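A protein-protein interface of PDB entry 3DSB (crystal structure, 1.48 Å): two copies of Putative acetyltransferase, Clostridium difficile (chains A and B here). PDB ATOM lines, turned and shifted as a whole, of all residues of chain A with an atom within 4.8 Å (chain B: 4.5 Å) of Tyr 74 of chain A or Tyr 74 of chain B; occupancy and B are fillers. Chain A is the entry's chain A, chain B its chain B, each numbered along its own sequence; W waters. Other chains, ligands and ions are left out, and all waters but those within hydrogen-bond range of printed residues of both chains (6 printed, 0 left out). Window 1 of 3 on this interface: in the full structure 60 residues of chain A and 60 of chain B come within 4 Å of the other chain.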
ATOM      1  N   GLU A  52      22.924  38.537  10.636  1.00  0.00           N
ATOM      2  CA  GLU A  52      22.791  37.340  11.462  1.00  0.00           C
ATOM      3  C   GLU A  52      22.040  36.204  10.743  1.00  0.00           C
ATOM      4  O   GLU A  52      22.128  35.024  11.130  1.00  0.00           O
ATOM      5  CB  GLU A  52      22.061  37.733  12.759  1.00  0.00           C
ATOM      6  CG  GLU A  52      20.750  38.577  12.531  1.00  0.00           C
ATOM      7  CD  GLU A  52      20.925  39.971  11.792  1.00  0.00           C
ATOM      8  OE1 GLU A  52      21.861  40.805  12.087  1.00  0.00           O
ATOM      9  OE2 GLU A  52      20.069  40.235  10.894  1.00  0.00           O
ATOM     10  N   ARG A  53      21.279  36.557   9.707  1.00  0.00           N
ATOM     11  CA  ARG A  53      20.584  35.561   8.931  1.00  0.00           C
ATOM     12  C   ARG A  53      21.528  34.767   8.044  1.00  0.00           C
ATOM     13  O   ARG A  53      21.182  33.651   7.631  1.00  0.00           O
ATOM     14  CB  ARG A  53      19.464  36.204   8.106  1.00  0.00           C
ATOM     15  CG  ARG A  53      18.435  36.912   8.978  1.00  0.00           C
ATOM     16  CD  ARG A  53      17.507  37.758   8.119  1.00  0.00           C
ATOM     17  NE  ARG A  53      18.154  38.970   7.608  1.00  0.00           N
ATOM     18  CZ  ARG A  53      17.569  39.832   6.769  1.00  0.00           C
ATOM     19  NH1 ARG A  53      16.339  39.606   6.312  1.00  0.00           N
ATOM     20  NH2 ARG A  53      18.220  40.915   6.363  1.00  0.00           N
ATOM     21  N   LYS A  54      22.722  35.307   7.754  1.00  0.00           N
ATOM     22  CA  LYS A  54      23.716  34.571   6.948  1.00  0.00           C
ATOM     23  C   LYS A  54      24.502  33.523   7.762  1.00  0.00           C
ATOM     24  O   LYS A  54      25.153  32.672   7.163  1.00  0.00           O
ATOM     25  CB  LYS A  54      24.707  35.522   6.291  1.00  0.00           C
ATOM     26  CG  LYS A  54      24.149  36.447   5.150  1.00  0.00           C
ATOM     27  CD  LYS A  54      25.226  37.335   4.537  1.00  0.00           C
ATOM     28  CE  LYS A  54      24.769  38.165   3.294  1.00  0.00           C
ATOM     29  NZ  LYS A  54      23.743  39.202   3.684  1.00  0.00           N
ATOM     30  N   GLY A  55      24.439  33.564   9.098  1.00  0.00           N
ATOM     31  CA  GLY A  55      25.347  32.755   9.924  1.00  0.00           C
ATOM     32  C   GLY A  55      25.881  33.598  11.066  1.00  0.00           C
ATOM     33  O   GLY A  55      25.497  34.775  11.238  1.00  0.00           O
ATOM     34  N   LYS A  56      26.756  33.005  11.860  1.00  0.00           N
ATOM     35  CA  LYS A  56      27.309  33.682  13.035  1.00  0.00           C
ATOM     36  C   LYS A  56      28.770  33.319  13.268  1.00  0.00           C
ATOM     37  O   LYS A  56      29.152  32.139  13.130  1.00  0.00           O
ATOM     38  CB  LYS A  56      26.537  33.284  14.302  1.00  0.00           C
ATOM     39  CG  LYS A  56      25.055  33.508  14.300  1.00  0.00           C
ATOM     40  CD  LYS A  56      24.648  34.941  14.523  1.00  0.00           C
ATOM     41  CE  LYS A  56      23.133  34.963  14.765  1.00  0.00           C
ATOM     42  NZ  LYS A  56      22.384  34.074  13.751  1.00  0.00           N
ATOM     43  N   TYR A  72      29.557  29.451  11.751  1.00  0.00           N
ATOM     44  CA  TYR A  72      28.584  28.516  11.160  1.00  0.00           C
ATOM     45  C   TYR A  72      27.547  29.230  10.338  1.00  0.00           C
ATOM     46  O   TYR A  72      27.246  30.413  10.573  1.00  0.00           O
ATOM     47  CB  TYR A  72      27.887  27.644  12.203  1.00  0.00           C
ATOM     48  CG  TYR A  72      27.133  28.382  13.271  1.00  0.00           C
ATOM     49  CD1 TYR A  72      25.843  28.875  13.050  1.00  0.00           C
ATOM     50  CD2 TYR A  72      27.700  28.593  14.530  1.00  0.00           C
ATOM     51  CE1 TYR A  72      25.133  29.558  14.056  1.00  0.00           C
ATOM     52  CE2 TYR A  72      27.012  29.229  15.530  1.00  0.00           C
ATOM     53  CZ  TYR A  72      25.738  29.724  15.305  1.00  0.00           C
ATOM     54  OH  TYR A  72      25.057  30.343  16.320  1.00  0.00           O
ATOM     55  N   THR A  73      26.996  28.484   9.381  1.00  0.00           N
ATOM     56  CA  THR A  73      25.844  28.950   8.621  1.00  0.00           C
ATOM     57  C   THR A  73      24.677  27.992   8.883  1.00  0.00           C
ATOM     58  O   THR A  73      24.835  26.978   9.562  1.00  0.00           O
ATOM     59  CB  THR A  73      26.144  28.953   7.115  1.00  0.00           C
ATOM     60  OG1 THR A  73      26.501  27.648   6.705  1.00  0.00           O
ATOM     61  CG2 THR A  73      27.282  29.893   6.732  1.00  0.00           C
ATOM     62  N   TYR A  74      23.516  28.294   8.281  1.00  0.00           N
ATOM     63  CA  TYR A  74      22.324  27.441   8.485  1.00  0.00           C
ATOM     64  C   TYR A  74      21.879  26.796   7.197  1.00  0.00           C
ATOM     65  O   TYR A  74      22.024  27.393   6.127  1.00  0.00           O
ATOM     66  CB  TYR A  74      21.124  28.277   8.908  1.00  0.00           C
ATOM     67  CG  TYR A  74      21.425  29.135  10.089  1.00  0.00           C
ATOM     68  CD1 TYR A  74      21.412  28.591  11.347  1.00  0.00           C
ATOM     69  CD2 TYR A  74      21.735  30.508   9.936  1.00  0.00           C
ATOM     70  CE1 TYR A  74      21.684  29.395  12.495  1.00  0.00           C
ATOM     71  CE2 TYR A  74      22.034  31.306  11.062  1.00  0.00           C
ATOM     72  CZ  TYR A  74      21.993  30.735  12.341  1.00  0.00           C
ATOM     73  OH  TYR A  74      22.263  31.502  13.457  1.00  0.00           O
ATOM     74  N   GLU A  75      21.294  25.603   7.332  1.00  0.00           N
ATOM     75  CA  GLU A  75      20.539  25.008   6.231  1.00  0.00           C
ATOM     76  C   GLU A  75      19.141  24.685   6.727  1.00  0.00           C
ATOM     77  O   GLU A  75      18.970  23.825   7.594  1.00  0.00           O
ATOM     78  CB  GLU A  75      21.193  23.684   5.809  1.00  0.00           C
ATOM     79  CG  GLU A  75      20.344  22.918   4.783  1.00  0.00           C
ATOM     80  CD  GLU A  75      20.725  21.442   4.633  1.00  0.00           C
ATOM     81  OE1 GLU A  75      21.819  21.033   5.073  1.00  0.00           O
ATOM     82  OE2 GLU A  75      19.891  20.691   4.090  1.00  0.00           O
ATOM     83  N   TRP A  76      18.126  25.380   6.185  1.00  0.00           N
ATOM     84  CA  TRP A  76      16.750  25.085   6.598  1.00  0.00           C
ATOM     85  C   TRP A  76      16.324  23.743   5.999  1.00  0.00           C
ATOM     86  O   TRP A  76      16.476  23.527   4.793  1.00  0.00           O
ATOM     87  CB  TRP A  76      15.793  26.180   6.121  1.00  0.00           C
ATOM     88  CG  TRP A  76      14.384  25.925   6.614  1.00  0.00           C
ATOM     89  CD1 TRP A  76      13.314  25.513   5.863  1.00  0.00           C
ATOM     90  CD2 TRP A  76      13.925  26.015   7.970  1.00  0.00           C
ATOM     91  NE1 TRP A  76      12.196  25.344   6.686  1.00  0.00           N
ATOM     92  CE2 TRP A  76      12.555  25.650   7.980  1.00  0.00           C
ATOM     93  CE3 TRP A  76      14.547  26.369   9.186  1.00  0.00           C
ATOM     94  CZ2 TRP A  76      11.798  25.649   9.158  1.00  0.00           C
ATOM     95  CZ3 TRP A  76      13.778  26.373  10.352  1.00  0.00           C
ATOM     96  CH2 TRP A  76      12.433  26.016  10.332  1.00  0.00           C
ATOM     97  N   ASN A  83      16.574  23.762  11.472  1.00  0.00           N
ATOM     98  CA  ASN A  83      17.843  24.105  10.825  1.00  0.00           C
ATOM     99  C   ASN A  83      18.900  23.069  11.129  1.00  0.00           C
ATOM    100  O   ASN A  83      18.998  22.604  12.288  1.00  0.00           O
ATOM    101  CB  ASN A  83      18.408  25.418  11.348  1.00  0.00           C
ATOM    102  CG  ASN A  83      17.826  26.621  10.674  1.00  0.00           C
ATOM    103  OD1 ASN A  83      17.210  27.484  11.354  1.00  0.00           O
ATOM    104  ND2 ASN A  83      17.968  26.715   9.382  1.00  0.00           N
ATOM    105  N   PHE A  84      19.724  22.752  10.123  1.00  0.00           N
ATOM    106  CA  PHE A  84      21.041  22.194  10.410  1.00  0.00           C
ATOM    107  C   PHE A  84      21.986  23.356  10.574  1.00  0.00           C
ATOM    108  O   PHE A  84      21.915  24.352   9.841  1.00  0.00           O
ATOM    109  CB  PHE A  84      21.509  21.384   9.214  1.00  0.00           C
ATOM    110  CG  PHE A  84      20.793  20.089   9.049  1.00  0.00           C
ATOM    111  CD1 PHE A  84      21.188  18.957   9.769  1.00  0.00           C
ATOM    112  CD2 PHE A  84      19.725  19.983   8.151  1.00  0.00           C
ATOM    113  CE1 PHE A  84      20.545  17.747   9.612  1.00  0.00           C
ATOM    114  CE2 PHE A  84      19.051  18.766   7.990  1.00  0.00           C
ATOM    115  CZ  PHE A  84      19.472  17.641   8.718  1.00  0.00           C
ATOM    116  N   TRP A  86      25.808  24.377  10.091  1.00  0.00           N
ATOM    117  CA  TRP A  86      26.998  23.892   9.358  1.00  0.00           C
ATOM    118  C   TRP A  86      28.211  24.680   9.836  1.00  0.00           C
ATOM    119  O   TRP A  86      28.301  25.884   9.620  1.00  0.00           O
ATOM    120  CB  TRP A  86      26.833  24.114   7.848  1.00  0.00           C
ATOM    121  CG  TRP A  86      25.938  23.153   7.196  1.00  0.00           C
ATOM    122  CD1 TRP A  86      24.570  23.119   7.233  1.00  0.00           C
ATOM    123  CD2 TRP A  86      26.353  21.962   6.486  1.00  0.00           C
ATOM    124  NE1 TRP A  86      24.097  22.027   6.502  1.00  0.00           N
ATOM    125  CE2 TRP A  86      25.172  21.317   6.017  1.00  0.00           C
ATOM    126  CE3 TRP A  86      27.597  21.457   6.086  1.00  0.00           C
ATOM    127  CZ2 TRP A  86      25.215  20.129   5.264  1.00  0.00           C
ATOM    128  CZ3 TRP A  86      27.634  20.273   5.362  1.00  0.00           C
ATOM    129  CH2 TRP A  86      26.456  19.637   4.937  1.00  0.00           C
ATOM    130  N   GLU B  52      12.559  34.459   2.783  1.00  0.00           N
ATOM    131  CA  GLU B  52      13.445  34.395   1.598  1.00  0.00           C
ATOM    132  C   GLU B  52      14.919  34.195   1.975  1.00  0.00           C
ATOM    133  O   GLU B  52      15.720  33.732   1.151  1.00  0.00           O
ATOM    134  CB  GLU B  52      13.314  35.686   0.776  1.00  0.00           C
ATOM    135  CG  GLU B  52      13.761  36.912   1.579  1.00  0.00           C
ATOM    136  CD  GLU B  52      14.060  38.124   0.721  1.00  0.00           C
ATOM    137  OE1 GLU B  52      13.335  38.328  -0.270  1.00  0.00           O
ATOM    138  OE2 GLU B  52      15.018  38.871   1.038  1.00  0.00           O
ATOM    139  N   ARG B  53      15.285  34.510   3.224  1.00  0.00           N
ATOM    140  CA  ARG B  53      16.678  34.326   3.642  1.00  0.00           C
ATOM    141  C   ARG B  53      16.999  32.858   3.908  1.00  0.00           C
ATOM    142  O   ARG B  53      18.193  32.462   3.916  1.00  0.00           O
ATOM    143  CB  ARG B  53      17.016  35.174   4.878  1.00  0.00           C
ATOM    144  CG  ARG B  53      16.573  36.620   4.722  1.00  0.00           C
ATOM    145  CD  ARG B  53      17.285  37.320   3.584  1.00  0.00           C
ATOM    146  NE  ARG B  53      18.683  36.902   3.520  1.00  0.00           N
ATOM    147  CZ  ARG B  53      19.684  37.530   4.133  1.00  0.00           C
ATOM    148  NH1 ARG B  53      20.916  37.073   4.021  1.00  0.00           N
ATOM    149  NH2 ARG B  53      19.455  38.628   4.839  1.00  0.00           N
ATOM    150  N   LYS B  54      15.954  32.041   4.094  1.00  0.00           N
ATOM    151  CA  LYS B  54      16.153  30.587   4.305  1.00  0.00           C
ATOM    152  C   LYS B  54      16.395  29.806   2.997  1.00  0.00           C
ATOM    153  O   LYS B  54      16.906  28.653   3.005  1.00  0.00           O
ATOM    154  CB  LYS B  54      14.973  29.952   5.039  1.00  0.00           C
ATOM    155  CG  LYS B  54      14.834  30.312   6.523  1.00  0.00           C
ATOM    156  CD  LYS B  54      13.619  29.616   7.141  1.00  0.00           C
ATOM    157  CE  LYS B  54      13.541  29.772   8.664  1.00  0.00           C
ATOM    158  NZ  LYS B  54      12.934  31.082   9.011  1.00  0.00           N
ATOM    159  N   GLY B  55      16.012  30.400   1.867  1.00  0.00           N
ATOM    160  CA  GLY B  55      16.100  29.679   0.566  1.00  0.00           C
ATOM    161  C   GLY B  55      14.886  30.046  -0.258  1.00  0.00           C
ATOM    162  O   GLY B  55      14.142  30.992   0.094  1.00  0.00           O
ATOM    163  N   LYS B  56      14.708  29.334  -1.359  1.00  0.00           N
ATOM    164  CA  LYS B  56      13.611  29.648  -2.285  1.00  0.00           C
ATOM    165  C   LYS B  56      13.111  28.393  -2.969  1.00  0.00           C
ATOM    166  O   LYS B  56      13.935  27.519  -3.337  1.00  0.00           O
ATOM    167  CB  LYS B  56      14.114  30.535  -3.417  1.00  0.00           C
ATOM    168  CG  LYS B  56      14.449  31.931  -3.072  1.00  0.00           C
ATOM    169  CD  LYS B  56      13.211  32.764  -2.969  1.00  0.00           C
ATOM    170  CE  LYS B  56      13.402  34.077  -3.677  1.00  0.00           C
ATOM    171  NZ  LYS B  56      14.657  34.753  -3.260  1.00  0.00           N
ATOM    172  N   TYR B  72      16.132  25.400  -3.126  1.00  0.00           N
ATOM    173  CA  TYR B  72      17.536  25.591  -2.689  1.00  0.00           C
ATOM    174  C   TYR B  72      17.632  26.449  -1.441  1.00  0.00           C
ATOM    175  O   TYR B  72      16.759  27.306  -1.168  1.00  0.00           O
ATOM    176  CB  TYR B  72      18.433  26.178  -3.782  1.00  0.00           C
ATOM    177  CG  TYR B  72      17.989  27.525  -4.334  1.00  0.00           C
ATOM    178  CD1 TYR B  72      18.255  28.712  -3.664  1.00  0.00           C
ATOM    179  CD2 TYR B  72      17.358  27.600  -5.581  1.00  0.00           C
ATOM    180  CE1 TYR B  72      17.856  29.951  -4.195  1.00  0.00           C
ATOM    181  CE2 TYR B  72      16.967  28.783  -6.131  1.00  0.00           C
ATOM    182  CZ  TYR B  72      17.212  29.966  -5.436  1.00  0.00           C
ATOM    183  OH  TYR B  72      16.848  31.186  -5.969  1.00  0.00           O
ATOM    184  N   THR B  73      18.703  26.195  -0.681  1.00  0.00           N
ATOM    185  CA  THR B  73      19.070  27.030   0.475  1.00  0.00           C
ATOM    186  C   THR B  73      20.366  27.766   0.138  1.00  0.00           C
ATOM    187  O   THR B  73      20.963  27.524  -0.917  1.00  0.00           O
ATOM    188  CB  THR B  73      19.269  26.203   1.734  1.00  0.00           C
ATOM    189  OG1 THR B  73      20.276  25.224   1.494  1.00  0.00           O
ATOM    190  CG2 THR B  73      17.951  25.498   2.143  1.00  0.00           C
ATOM    191  N   TYR B  74      20.831  28.613   1.060  1.00  0.00           N
ATOM    192  CA  TYR B  74      22.059  29.377   0.826  1.00  0.00           C
ATOM    193  C   TYR B  74      23.124  29.009   1.824  1.00  0.00           C
ATOM    194  O   TYR B  74      22.806  28.683   2.986  1.00  0.00           O
ATOM    195  CB  TYR B  74      21.795  30.872   1.051  1.00  0.00           C
ATOM    196  CG  TYR B  74      20.730  31.432   0.145  1.00  0.00           C
ATOM    197  CD1 TYR B  74      20.992  31.676  -1.194  1.00  0.00           C
ATOM    198  CD2 TYR B  74      19.481  31.770   0.646  1.00  0.00           C
ATOM    199  CE1 TYR B  74      20.011  32.218  -2.042  1.00  0.00           C
ATOM    200  CE2 TYR B  74      18.499  32.328  -0.190  1.00  0.00           C
ATOM    201  CZ  TYR B  74      18.766  32.525  -1.524  1.00  0.00           C
ATOM    202  OH  TYR B  74      17.771  33.109  -2.303  1.00  0.00           O
ATOM    203  N   GLU B  75      24.371  29.034   1.370  1.00  0.00           N
ATOM    204  CA  GLU B  75      25.476  29.033   2.327  1.00  0.00           C
ATOM    205  C   GLU B  75      26.349  30.255   2.009  1.00  0.00           C
ATOM    206  O   GLU B  75      26.979  30.327   0.957  1.00  0.00           O
ATOM    207  CB  GLU B  75      26.316  27.773   2.114  1.00  0.00           C
ATOM    208  CG  GLU B  75      27.622  27.818   2.932  1.00  0.00           C
ATOM    209  CD  GLU B  75      28.711  26.885   2.396  1.00  0.00           C
ATOM    210  OE1 GLU B  75      28.416  25.915   1.686  1.00  0.00           O
ATOM    211  OE2 GLU B  75      29.900  27.129   2.714  1.00  0.00           O
ATOM    212  N   TRP B  76      26.395  31.213   2.941  1.00  0.00           N
ATOM    213  CA  TRP B  76      27.266  32.392   2.751  1.00  0.00           C
ATOM    214  C   TRP B  76      28.727  31.945   2.865  1.00  0.00           C
ATOM    215  O   TRP B  76      29.097  31.315   3.858  1.00  0.00           O
ATOM    216  CB  TRP B  76      26.953  33.483   3.784  1.00  0.00           C
ATOM    217  CG  TRP B  76      27.791  34.713   3.527  1.00  0.00           C
ATOM    218  CD1 TRP B  76      28.923  35.138   4.225  1.00  0.00           C
ATOM    219  CD2 TRP B  76      27.614  35.633   2.457  1.00  0.00           C
ATOM    220  NE1 TRP B  76      29.452  36.284   3.617  1.00  0.00           N
ATOM    221  CE2 TRP B  76      28.673  36.598   2.527  1.00  0.00           C
ATOM    222  CE3 TRP B  76      26.690  35.715   1.411  1.00  0.00           C
ATOM    223  CZ2 TRP B  76      28.770  37.677   1.628  1.00  0.00           C
ATOM    224  CZ3 TRP B  76      26.779  36.806   0.516  1.00  0.00           C
ATOM    225  CH2 TRP B  76      27.828  37.743   0.611  1.00  0.00           C
ATOM    226  N   ASN B  83      27.178  33.732  -1.976  1.00  0.00           N
ATOM    227  CA  ASN B  83      26.459  32.539  -1.553  1.00  0.00           C
ATOM    228  C   ASN B  83      26.746  31.378  -2.474  1.00  0.00           C
ATOM    229  O   ASN B  83      26.778  31.545  -3.719  1.00  0.00           O
ATOM    230  CB  ASN B  83      24.957  32.781  -1.620  1.00  0.00           C
ATOM    231  CG  ASN B  83      24.430  33.523  -0.418  1.00  0.00           C
ATOM    232  OD1 ASN B  83      24.589  33.092   0.725  1.00  0.00           O
ATOM    233  ND2 ASN B  83      23.750  34.648  -0.667  1.00  0.00           N
ATOM    234  N   PHE B  84      26.875  30.185  -1.888  1.00  0.00           N
ATOM    235  CA  PHE B  84      26.626  28.981  -2.661  1.00  0.00           C
ATOM    236  C   PHE B  84      25.132  28.743  -2.576  1.00  0.00           C
ATOM    237  O   PHE B  84      24.537  28.889  -1.517  1.00  0.00           O
ATOM    238  CB  PHE B  84      27.323  27.780  -2.015  1.00  0.00           C
ATOM    239  CG  PHE B  84      28.784  27.782  -2.166  1.00  0.00           C
ATOM    240  CD1 PHE B  84      29.387  27.266  -3.302  1.00  0.00           C
ATOM    241  CD2 PHE B  84      29.598  28.304  -1.131  1.00  0.00           C
ATOM    242  CE1 PHE B  84      30.768  27.270  -3.480  1.00  0.00           C
ATOM    243  CE2 PHE B  84      30.973  28.325  -1.277  1.00  0.00           C
ATOM    244  CZ  PHE B  84      31.569  27.799  -2.465  1.00  0.00           C
ATOM    245  N   LEU B  85      24.527  28.320  -3.686  1.00  0.00           N
ATOM    246  CA  LEU B  85      23.171  27.764  -3.630  1.00  0.00           C
ATOM    247  C   LEU B  85      23.271  26.250  -3.499  1.00  0.00           C
ATOM    248  O   LEU B  85      24.034  25.617  -4.244  1.00  0.00           O
ATOM    249  CB  LEU B  85      22.389  28.071  -4.916  1.00  0.00           C
ATOM    250  CG  LEU B  85      21.589  29.365  -4.969  1.00  0.00           C
ATOM    251  CD1 LEU B  85      22.284  30.571  -4.417  1.00  0.00           C
ATOM    252  CD2 LEU B  85      20.929  29.577  -6.354  1.00  0.00           C
HETATM  253  O   HOH W   1      24.625  26.735   5.103  1.00  0.00           O
HETATM  254  O   HOH W   2      22.242  25.836   3.055  1.00  0.00           O
HETATM  255  O   HOH W   3      20.265  31.714   6.067  1.00  0.00           O
HETATM  256  O   HOH W   4      24.384  31.482   4.924  1.00  0.00           O
HETATM  257  O   HOH W   5      18.583  27.844   4.948  1.00  0.00           O
HETATM  258  O   HOH W   6      22.350  30.032   6.070  1.00  0.00           O
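The side-chain amino group (NZ) of Lys 56 of chain A sits at hydrogen-bond distance from the side-chain hydroxyl (OH) of Tyr 74 of chain A (2.6 Å). O of Thr 73 of chain A is in hydrogen-bond range of N of Trp 86 of chain A (2.8 Å). The backbone NH of Trp 76 of chain A sits close to the side-chain amide nitrogen of Asn 83 of chain A (3.5 Å). O of Glu 75 of chain B sits at hydrogen-bond distance from N of Phe 84 of chain B (2.9 Å). The side-chain amide oxygen of Asn 83 of chain B lies within hydrogen-bond range of the backbone NH of Trp 76 of chain B (3.4 Å).
Arg 53 of chain B touches its own counterpart, Arg 53 of chain A. Lys 54 of chain A touches Arg 53 of chain B, but with the chains exchanged Arg 53 of chain A does not touch Lys 54 of chain B (6.5 Å). Thr 73 of chain A touches Glu 75 of chain B, but with the chains exchanged Glu 75 of chain A does not touch Thr 73 of chain B (4.02 Å). Tyr 74 of chain A touches its own counterpart, Tyr 74 of chain B. Positions printed for both chains: 52, 53, 54, 55, 56, 72, 73, 74, 75, 76, 83 and 84.
Of chain A, only Tyr 74 comes within 4 Å of Tyr 74 of chain B. Of the printed residues of chain A, Glu 75 of chain B touches Thr 73 (3.9 Å). Of the printed residues of chain A, Trp 76 of chain B touches Lys 54 and Thr 73. Of the printed residues of chain A, Lys 54 of chain B touches Trp 76 (3.6 Å). Of the printed residues of chain B, Lys 54 of chain A touches Arg 53 and Trp 76. Printed residues of chain A within 4 Å of Arg 53 of chain B: Arg 53 and Lys 54. Glu 75 of chain A touches none of the printed residues of chain B. Asn 83 of chain B touches none of the printed residues of chain A.
Among the printed residues, pairs that only touch across the chains: Lys 54 of chain A with Arg 53 of chain B (3.5 Å), Lys 54 of chain A with Trp 76 of chain B (3.6 Å), Thr 73 of chain A with Glu 75 of chain B (3.9 Å), Thr 73 of chain A with Trp 76 of chain B (3.7 Å), Trp 76 of chain A with Lys 54 of chain B (3.6 Å) and Trp 76 of chain A with Thr 73 of chain B (3.6 Å).
The guanidinium group (NH2) of Arg 53 of chain A lies close to the guanidinium group (NH2) of Arg 53 of chain B, 3.0 Å away. The backbone carbonyl oxygen (O) of Tyr 74 of chain A sits close to the backbone carbonyl oxygen (O) of Tyr 74 of chain B, 3.5 Å away.
Of the 13 printed residues of chain B, 6 touch a printed residue of chain A. Hydrophobic or aromatic side chains of chain B within 4 Å of the printed part of chain A: Trp 76.
Water W2 lies within hydrogen-bond range of the side-chain hydroxyl (OG1) of Thr 73 of chain B (2.6 Å), the backbone carbonyl oxygen (O) of Tyr 74 of chain B (2.9 Å) and the backbone carbonyl oxygen (O) of Tyr 74 of chain A (3.5 Å). Water W1 lies within hydrogen-bond range of the side-chain hydroxyl (OG1) of Thr 73 of chain A (2.6 Å), the backbone carbonyl oxygen (O) of Tyr 74 of chain A (2.9 Å) and the backbone carbonyl oxygen (O) of Tyr 74 of chain B (3.4 Å). Water W4 bridges O of Lys 54 of chain A and N of Trp 76 of chain B. Water W3 lies within hydrogen-bond range of O of Arg 53 of chain A (2.7 Å) and O of Arg 53 of chain B (3.1 Å). Water W6 lies within hydrogen-bond range of O of Tyr 74 of chain A and O of Tyr 74 of chain B. Water W5 bridges O of Lys 54 of chain B (2.7 Å) and N of Trp 76 of chain A (2.8 Å).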
